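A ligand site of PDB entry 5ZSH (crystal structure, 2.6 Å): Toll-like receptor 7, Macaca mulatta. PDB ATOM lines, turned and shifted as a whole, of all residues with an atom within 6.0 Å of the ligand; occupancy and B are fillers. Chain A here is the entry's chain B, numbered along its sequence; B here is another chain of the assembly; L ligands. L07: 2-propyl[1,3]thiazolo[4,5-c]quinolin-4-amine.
The side-chain carboxylate (OD2) of Asp 533 lies within hydrogen-bond range of a nitrogen (N1) of the ligand, at 2.6 Å. The backbone NH of Thr 564 sits at hydrogen-bond distance from a nitrogen (N2) of the ligand (3.3 Å). The backbone carbonyl oxygen (O) of Thr 564 sits at hydrogen-bond distance from a nitrogen (N) of the ligand, 3.3 Å away.
The backbone carbonyl oxygen (O) of Phe 386 of chain B lies within hydrogen-bond range of the side-chain hydroxyl (OH) of Tyr 334 of chain B. ND2 of Asn 243 of chain B lies within hydrogen-bond range of OG1 of Thr 564 (2.8 Å). The side-chain hydroxyl (OG1) of Thr 564 lies within hydrogen-bond range of the side-chain hydroxyl (OH) of Tyr 242 of chain B (3.3 Å). O of Ile 563 sits close to ND1 of His 565, at 3.2 Å. O of Gly 357 of chain B lies close to N of Phe 329 of chain B. The backbone NH (N) of Val 359 of chain B lies within hydrogen-bond range of the side-chain amide oxygen (OD1) of Asn 385 of chain B, at 2.8 Å.
CG2 of Thr 510 touches C12 of the ligand (3.7 Å). Leu 535 touches the ligand (CD2 to C1, 3.5 Å). Gly 562 touches the ligand. Ile 563 touches the ligand (CG2 to N, 3.3 Å). Phe 327 of chain B touches the ligand (CE1 to C8, 3.4 Å). Phe 329 of chain B touches the ligand. Tyr 334 of chain B touches the ligand (CE2 to C10, 3.4 Å). Val 359 of chain B touches the ligand. Phe 386 of chain B touches the ligand (CZ to C4, 3.2 Å). Hydrophobic or aromatic side chains that line the ligand: Leu 535, Ile 563, Phe 327 of chain B, Phe 329 of chain B, Tyr 334 of chain B, Val 359 of chain B and Phe 386 of chain B. 11 residues have an atom within 4 Å of the ligand: Thr 510, Asp 533, Leu 535, Gly 562, Ile 563, Thr 564, Phe 327 of chain B, Phe 329 of chain B, Tyr 334 of chain B, Val 359 of chain B and Phe 386 of chain B. The nearest printed residue that does not touch the ligand is Asn 243 of chain B (4.5 Å).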
ATOM      1  N   THR A 510       2.058 -12.336 -10.873  1.00  0.00           N
ATOM      2  CA  THR A 510       3.227 -12.449 -11.739  1.00  0.00           C
ATOM      3  C   THR A 510       3.721 -13.892 -11.693  1.00  0.00           C
ATOM      4  O   THR A 510       3.837 -14.479 -10.613  1.00  0.00           O
ATOM      5  CB  THR A 510       4.337 -11.491 -11.326  1.00  0.00           C
ATOM      6  OG1 THR A 510       5.046 -12.058 -10.223  1.00  0.00           O
ATOM      7  CG2 THR A 510       3.797 -10.132 -10.906  1.00  0.00           C
ATOM      8  N   ASP A 533       0.287 -11.066 -15.142  1.00  0.00           N
ATOM      9  CA  ASP A 533       1.213  -9.935 -15.043  1.00  0.00           C
ATOM     10  C   ASP A 533       2.589 -10.405 -15.489  1.00  0.00           C
ATOM     11  O   ASP A 533       3.297 -11.073 -14.719  1.00  0.00           O
ATOM     12  CB  ASP A 533       1.267  -9.370 -13.642  1.00  0.00           C
ATOM     13  CG  ASP A 533       2.164  -8.147 -13.542  1.00  0.00           C
ATOM     14  OD1 ASP A 533       2.720  -7.675 -14.566  1.00  0.00           O
ATOM     15  OD2 ASP A 533       2.364  -7.647 -12.423  1.00  0.00           O
ATOM     16  N   LEU A 534       2.975 -10.021 -16.703  1.00  0.00           N
ATOM     17  CA  LEU A 534       4.282 -10.379 -17.262  1.00  0.00           C
ATOM     18  C   LEU A 534       5.399  -9.454 -16.770  1.00  0.00           C
ATOM     19  O   LEU A 534       6.062  -8.770 -17.537  1.00  0.00           O
ATOM     20  CB  LEU A 534       4.194 -10.371 -18.785  1.00  0.00           C
ATOM     21  CG  LEU A 534       3.598 -11.664 -19.367  1.00  0.00           C
ATOM     22  CD1 LEU A 534       3.238 -11.428 -20.819  1.00  0.00           C
ATOM     23  CD2 LEU A 534       4.553 -12.854 -19.213  1.00  0.00           C
ATOM     24  N   LEU A 535       5.625  -9.474 -15.449  1.00  0.00           N
ATOM     25  CA  LEU A 535       6.749  -8.745 -14.869  1.00  0.00           C
ATOM     26  C   LEU A 535       8.085  -9.391 -15.216  1.00  0.00           C
ATOM     27  O   LEU A 535       9.077  -8.688 -15.445  1.00  0.00           O
ATOM     28  CB  LEU A 535       6.601  -8.672 -13.356  1.00  0.00           C
ATOM     29  CG  LEU A 535       7.744  -8.034 -12.572  1.00  0.00           C
ATOM     30  CD1 LEU A 535       8.084  -6.648 -13.125  1.00  0.00           C
ATOM     31  CD2 LEU A 535       7.397  -7.940 -11.077  1.00  0.00           C
ATOM     32  N   TYR A 557      -3.490  -5.643 -16.596  1.00  0.00           N
ATOM     33  CA  TYR A 557      -2.272  -4.887 -16.319  1.00  0.00           C
ATOM     34  C   TYR A 557      -1.735  -4.143 -17.544  1.00  0.00           C
ATOM     35  O   TYR A 557      -0.829  -3.314 -17.371  1.00  0.00           O
ATOM     36  CB  TYR A 557      -1.190  -5.796 -15.744  1.00  0.00           C
ATOM     37  CG  TYR A 557      -1.446  -6.203 -14.325  1.00  0.00           C
ATOM     38  CD1 TYR A 557      -1.329  -5.284 -13.268  1.00  0.00           C
ATOM     39  CD2 TYR A 557      -1.788  -7.513 -14.015  1.00  0.00           C
ATOM     40  CE1 TYR A 557      -1.561  -5.673 -11.939  1.00  0.00           C
ATOM     41  CE2 TYR A 557      -2.015  -7.908 -12.709  1.00  0.00           C
ATOM     42  CZ  TYR A 557      -1.913  -6.991 -11.668  1.00  0.00           C
ATOM     43  OH  TYR A 557      -2.146  -7.413 -10.369  1.00  0.00           O
ATOM     44  N   GLU A 561      -1.161   2.778 -17.440  1.00  0.00           N
ATOM     45  CA  GLU A 561       0.106   3.260 -17.964  1.00  0.00           C
ATOM     46  C   GLU A 561       1.269   2.994 -17.005  1.00  0.00           C
ATOM     47  O   GLU A 561       1.095   2.949 -15.781  1.00  0.00           O
ATOM     48  CB  GLU A 561       0.049   4.755 -18.205  1.00  0.00           C
ATOM     49  CG  GLU A 561      -0.145   5.502 -16.899  1.00  0.00           C
ATOM     50  CD  GLU A 561       0.196   6.973 -16.977  1.00  0.00           C
ATOM     51  OE1 GLU A 561      -0.232   7.693 -16.068  1.00  0.00           O
ATOM     52  OE2 GLU A 561       0.856   7.389 -17.967  1.00  0.00           O
ATOM     53  N   GLY A 562       2.463   2.836 -17.575  1.00  0.00           N
ATOM     54  CA  GLY A 562       3.673   2.812 -16.807  1.00  0.00           C
ATOM     55  C   GLY A 562       4.063   1.473 -16.263  1.00  0.00           C
ATOM     56  O   GLY A 562       5.066   1.376 -15.552  1.00  0.00           O
ATOM     57  N   ILE A 563       3.298   0.449 -16.510  1.00  0.00           N
ATOM     58  CA  ILE A 563       3.524  -0.852 -15.919  1.00  0.00           C
ATOM     59  C   ILE A 563       4.443  -1.678 -16.799  1.00  0.00           C
ATOM     60  O   ILE A 563       4.382  -1.615 -18.036  1.00  0.00           O
ATOM     61  CB  ILE A 563       2.182  -1.563 -15.663  1.00  0.00           C
ATOM     62  CG1 ILE A 563       1.402  -0.749 -14.627  1.00  0.00           C
ATOM     63  CG2 ILE A 563       2.369  -3.017 -15.215  1.00  0.00           C
ATOM     64  CD1 ILE A 563       0.029  -1.322 -14.299  1.00  0.00           C
ATOM     65  N   THR A 564       5.316  -2.436 -16.163  1.00  0.00           N
ATOM     66  CA  THR A 564       6.311  -3.233 -16.864  1.00  0.00           C
ATOM     67  C   THR A 564       5.694  -4.487 -17.495  1.00  0.00           C
ATOM     68  O   THR A 564       4.997  -5.245 -16.822  1.00  0.00           O
ATOM     69  CB  THR A 564       7.401  -3.626 -15.883  1.00  0.00           C
ATOM     70  OG1 THR A 564       8.100  -2.436 -15.485  1.00  0.00           O
ATOM     71  CG2 THR A 564       8.374  -4.552 -16.523  1.00  0.00           C
ATOM     72  N   HIS A 565       6.020  -4.746 -18.756  1.00  0.00           N
ATOM     73  CA  HIS A 565       5.491  -5.897 -19.495  1.00  0.00           C
ATOM     74  C   HIS A 565       6.642  -6.526 -20.248  1.00  0.00           C
ATOM     75  O   HIS A 565       7.233  -5.892 -21.118  1.00  0.00           O
ATOM     76  CB  HIS A 565       4.383  -5.487 -20.479  1.00  0.00           C
ATOM     77  CG  HIS A 565       3.307  -4.658 -19.861  1.00  0.00           C
ATOM     78  ND1 HIS A 565       2.956  -3.401 -20.338  1.00  0.00           N
ATOM     79  CD2 HIS A 565       2.494  -4.895 -18.808  1.00  0.00           C
ATOM     80  CE1 HIS A 565       1.994  -2.899 -19.596  1.00  0.00           C
ATOM     81  NE2 HIS A 565       1.687  -3.778 -18.667  1.00  0.00           N
ATOM     82  N   TYR B 242      12.701   4.730 -18.179  1.00  0.00           N
ATOM     83  CA  TYR B 242      12.190   3.386 -17.943  1.00  0.00           C
ATOM     84  C   TYR B 242      10.705   3.318 -18.322  1.00  0.00           C
ATOM     85  O   TYR B 242       9.895   4.117 -17.833  1.00  0.00           O
ATOM     86  CB  TYR B 242      12.398   3.002 -16.477  1.00  0.00           C
ATOM     87  CG  TYR B 242      12.088   1.550 -16.182  1.00  0.00           C
ATOM     88  CD1 TYR B 242      12.818   0.549 -16.800  1.00  0.00           C
ATOM     89  CD2 TYR B 242      11.083   1.190 -15.286  1.00  0.00           C
ATOM     90  CE1 TYR B 242      12.557  -0.785 -16.552  1.00  0.00           C
ATOM     91  CE2 TYR B 242      10.821  -0.148 -15.024  1.00  0.00           C
ATOM     92  CZ  TYR B 242      11.562  -1.131 -15.674  1.00  0.00           C
ATOM     93  OH  TYR B 242      11.351  -2.466 -15.431  1.00  0.00           O
ATOM     94  N   ASN B 243      10.360   2.377 -19.211  1.00  0.00           N
ATOM     95  CA  ASN B 243       8.991   2.194 -19.703  1.00  0.00           C
ATOM     96  C   ASN B 243       8.428   3.459 -20.369  1.00  0.00           C
ATOM     97  O   ASN B 243       7.223   3.737 -20.310  1.00  0.00           O
ATOM     98  CB  ASN B 243       8.063   1.713 -18.587  1.00  0.00           C
ATOM     99  CG  ASN B 243       8.275   0.253 -18.257  1.00  0.00           C
ATOM    100  OD1 ASN B 243       8.687  -0.538 -19.127  1.00  0.00           O
ATOM    101  ND2 ASN B 243       8.046  -0.118 -16.996  1.00  0.00           N
ATOM    102  N   PHE B 327       5.838   7.935  -9.420  1.00  0.00           N
ATOM    103  CA  PHE B 327       6.828   7.181 -10.198  1.00  0.00           C
ATOM    104  C   PHE B 327       8.233   7.681  -9.892  1.00  0.00           C
ATOM    105  O   PHE B 327       8.930   8.242 -10.741  1.00  0.00           O
ATOM    106  CB  PHE B 327       6.521   7.247 -11.699  1.00  0.00           C
ATOM    107  CG  PHE B 327       5.230   6.586 -12.064  1.00  0.00           C
ATOM    108  CD1 PHE B 327       5.152   5.205 -12.201  1.00  0.00           C
ATOM    109  CD2 PHE B 327       4.072   7.329 -12.233  1.00  0.00           C
ATOM    110  CE1 PHE B 327       3.954   4.595 -12.527  1.00  0.00           C
ATOM    111  CE2 PHE B 327       2.868   6.725 -12.535  1.00  0.00           C
ATOM    112  CZ  PHE B 327       2.808   5.354 -12.684  1.00  0.00           C
ATOM    113  N   PHE B 329      10.086   5.315  -8.012  1.00  0.00           N
ATOM    114  CA  PHE B 329      10.600   4.067  -7.482  1.00  0.00           C
ATOM    115  C   PHE B 329      11.970   3.705  -8.047  1.00  0.00           C
ATOM    116  O   PHE B 329      12.323   4.034  -9.183  1.00  0.00           O
ATOM    117  CB  PHE B 329       9.605   2.936  -7.753  1.00  0.00           C
ATOM    118  CG  PHE B 329       9.501   2.537  -9.214  1.00  0.00           C
ATOM    119  CD1 PHE B 329       8.719   3.267 -10.102  1.00  0.00           C
ATOM    120  CD2 PHE B 329      10.144   1.400  -9.682  1.00  0.00           C
ATOM    121  CE1 PHE B 329       8.610   2.896 -11.425  1.00  0.00           C
ATOM    122  CE2 PHE B 329      10.043   1.030 -11.012  1.00  0.00           C
ATOM    123  CZ  PHE B 329       9.276   1.762 -11.883  1.00  0.00           C
ATOM    124  N   TYR B 334      11.037  -3.714  -4.690  1.00  0.00           N
ATOM    125  CA  TYR B 334       9.661  -3.824  -4.227  1.00  0.00           C
ATOM    126  C   TYR B 334       9.695  -3.537  -2.724  1.00  0.00           C
ATOM    127  O   TYR B 334       9.843  -4.455  -1.905  1.00  0.00           O
ATOM    128  CB  TYR B 334       9.093  -5.205  -4.552  1.00  0.00           C
ATOM    129  CG  TYR B 334       7.584  -5.357  -4.399  1.00  0.00           C
ATOM    130  CD1 TYR B 334       6.746  -4.252  -4.189  1.00  0.00           C
ATOM    131  CD2 TYR B 334       6.993  -6.609  -4.472  1.00  0.00           C
ATOM    132  CE1 TYR B 334       5.369  -4.399  -4.057  1.00  0.00           C
ATOM    133  CE2 TYR B 334       5.627  -6.773  -4.329  1.00  0.00           C
ATOM    134  CZ  TYR B 334       4.815  -5.683  -4.123  1.00  0.00           C
ATOM    135  OH  TYR B 334       3.450  -5.900  -3.980  1.00  0.00           O
ATOM    136  N   GLY B 357       3.159   4.871  -8.078  1.00  0.00           N
ATOM    137  CA  GLY B 357       4.408   4.259  -8.515  1.00  0.00           C
ATOM    138  C   GLY B 357       5.552   4.433  -7.552  1.00  0.00           C
ATOM    139  O   GLY B 357       6.706   4.584  -7.969  1.00  0.00           O
ATOM    140  N   VAL B 359       5.607   1.931  -5.284  1.00  0.00           N
ATOM    141  CA  VAL B 359       5.759   0.476  -5.431  1.00  0.00           C
ATOM    142  C   VAL B 359       6.165  -0.166  -4.097  1.00  0.00           C
ATOM    143  O   VAL B 359       7.360  -0.333  -3.806  1.00  0.00           O
ATOM    144  CB  VAL B 359       6.757   0.121  -6.550  1.00  0.00           C
ATOM    145  CG1 VAL B 359       6.811  -1.404  -6.785  1.00  0.00           C
ATOM    146  CG2 VAL B 359       6.431   0.849  -7.844  1.00  0.00           C
ATOM    147  N   THR B 384      -1.513   2.752  -8.546  1.00  0.00           N
ATOM    148  CA  THR B 384      -0.405   2.096  -9.242  1.00  0.00           C
ATOM    149  C   THR B 384       0.805   1.966  -8.319  1.00  0.00           C
ATOM    150  O   THR B 384       1.904   2.451  -8.585  1.00  0.00           O
ATOM    151  CB  THR B 384      -0.044   2.837 -10.533  1.00  0.00           C
ATOM    152  OG1 THR B 384      -1.244   3.172 -11.241  1.00  0.00           O
ATOM    153  CG2 THR B 384       0.848   1.989 -11.427  1.00  0.00           C
ATOM    154  N   ASN B 385       0.578   1.307  -7.176  1.00  0.00           N
ATOM    155  CA  ASN B 385       1.640   1.076  -6.220  1.00  0.00           C
ATOM    156  C   ASN B 385       1.857  -0.394  -5.900  1.00  0.00           C
ATOM    157  O   ASN B 385       2.827  -0.714  -5.197  1.00  0.00           O
ATOM    158  CB  ASN B 385       1.373   1.856  -4.930  1.00  0.00           C
ATOM    159  CG  ASN B 385       1.987   3.247  -4.959  1.00  0.00           C
ATOM    160  OD1 ASN B 385       3.193   3.386  -5.180  1.00  0.00           O
ATOM    161  ND2 ASN B 385       1.161   4.280  -4.767  1.00  0.00           N
ATOM    162  N   PHE B 386       1.022  -1.288  -6.445  1.00  0.00           N
ATOM    163  CA  PHE B 386       1.085  -2.726  -6.182  1.00  0.00           C
ATOM    164  C   PHE B 386       0.990  -3.042  -4.696  1.00  0.00           C
ATOM    165  O   PHE B 386       1.595  -3.995  -4.196  1.00  0.00           O
ATOM    166  CB  PHE B 386       2.333  -3.351  -6.805  1.00  0.00           C
ATOM    167  CG  PHE B 386       2.325  -3.319  -8.289  1.00  0.00           C
ATOM    168  CD1 PHE B 386       1.764  -4.359  -9.015  1.00  0.00           C
ATOM    169  CD2 PHE B 386       2.826  -2.224  -8.970  1.00  0.00           C
ATOM    170  CE1 PHE B 386       1.736  -4.326 -10.405  1.00  0.00           C
ATOM    171  CE2 PHE B 386       2.799  -2.186 -10.344  1.00  0.00           C
ATOM    172  CZ  PHE B 386       2.247  -3.251 -11.061  1.00  0.00           C
ATOM    173  N   LYS B 410      -3.051  -4.174  -5.641  1.00  0.00           N
ATOM    174  CA  LYS B 410      -3.350  -5.598  -5.462  1.00  0.00           C
ATOM    175  C   LYS B 410      -3.957  -5.855  -4.084  1.00  0.00           C
ATOM    176  O   LYS B 410      -3.765  -6.931  -3.508  1.00  0.00           O
ATOM    177  CB  LYS B 410      -2.099  -6.463  -5.672  1.00  0.00           C
ATOM    178  CG  LYS B 410      -1.477  -6.326  -7.052  1.00  0.00           C
ATOM    179  CD  LYS B 410      -0.236  -7.199  -7.301  1.00  0.00           C
ATOM    180  CE  LYS B 410      -0.519  -8.683  -7.423  1.00  0.00           C
ATOM    181  NZ  LYS B 410       0.773  -9.447  -7.532  1.00  0.00           N
ATOM    182  N   PHE B 444       3.116   9.117 -18.205  1.00  0.00           N
ATOM    183  CA  PHE B 444       4.013   8.511 -19.175  1.00  0.00           C
ATOM    184  C   PHE B 444       3.851   9.052 -20.591  1.00  0.00           C
ATOM    185  O   PHE B 444       4.644   8.701 -21.461  1.00  0.00           O
ATOM    186  CB  PHE B 444       3.842   6.997 -19.167  1.00  0.00           C
ATOM    187  CG  PHE B 444       4.547   6.346 -18.028  1.00  0.00           C
ATOM    188  CD1 PHE B 444       5.816   5.800 -18.213  1.00  0.00           C
ATOM    189  CD2 PHE B 444       3.974   6.332 -16.754  1.00  0.00           C
ATOM    190  CE1 PHE B 444       6.495   5.199 -17.157  1.00  0.00           C
ATOM    191  CE2 PHE B 444       4.643   5.750 -15.678  1.00  0.00           C
ATOM    192  CZ  PHE B 444       5.905   5.175 -15.871  1.00  0.00           C
HETATM  193  C7  L07 L   1       5.613   0.199 -12.092  1.00  0.00           C
HETATM  194  C8  L07 L   1       5.661   1.629 -12.543  1.00  0.00           C
HETATM  195  C12 L07 L   1       4.404  -6.931  -9.241  1.00  0.00           C
HETATM  196  C11 L07 L   1       4.853  -6.747  -7.931  1.00  0.00           C
HETATM  197  C10 L07 L   1       5.548  -5.603  -7.553  1.00  0.00           C
HETATM  198  C9  L07 L   1       5.828  -4.591  -8.476  1.00  0.00           C
HETATM  199  N2  L07 L   1       5.510  -2.910 -12.937  1.00  0.00           N
HETATM  200  N1  L07 L   1       4.244  -6.126 -11.480  1.00  0.00           N
HETATM  201  N   L07 L   1       4.012  -5.408 -13.723  1.00  0.00           N
HETATM  202  C2  L07 L   1       5.409  -4.737  -9.797  1.00  0.00           C
HETATM  203  C3  L07 L   1       5.642  -3.796 -10.771  1.00  0.00           C
HETATM  204  C4  L07 L   1       5.171  -3.975 -12.161  1.00  0.00           C
HETATM  205  C5  L07 L   1       6.212  -1.971 -12.282  1.00  0.00           C
HETATM  206  C6  L07 L   1       6.741  -0.631 -12.715  1.00  0.00           C
HETATM  207  C1  L07 L   1       4.666  -5.959 -10.198  1.00  0.00           C
HETATM  208  C   L07 L   1       4.447  -5.215 -12.470  1.00  0.00           C
HETATM  209  S   L07 L   1       6.435  -2.343 -10.600  1.00  0.00           S
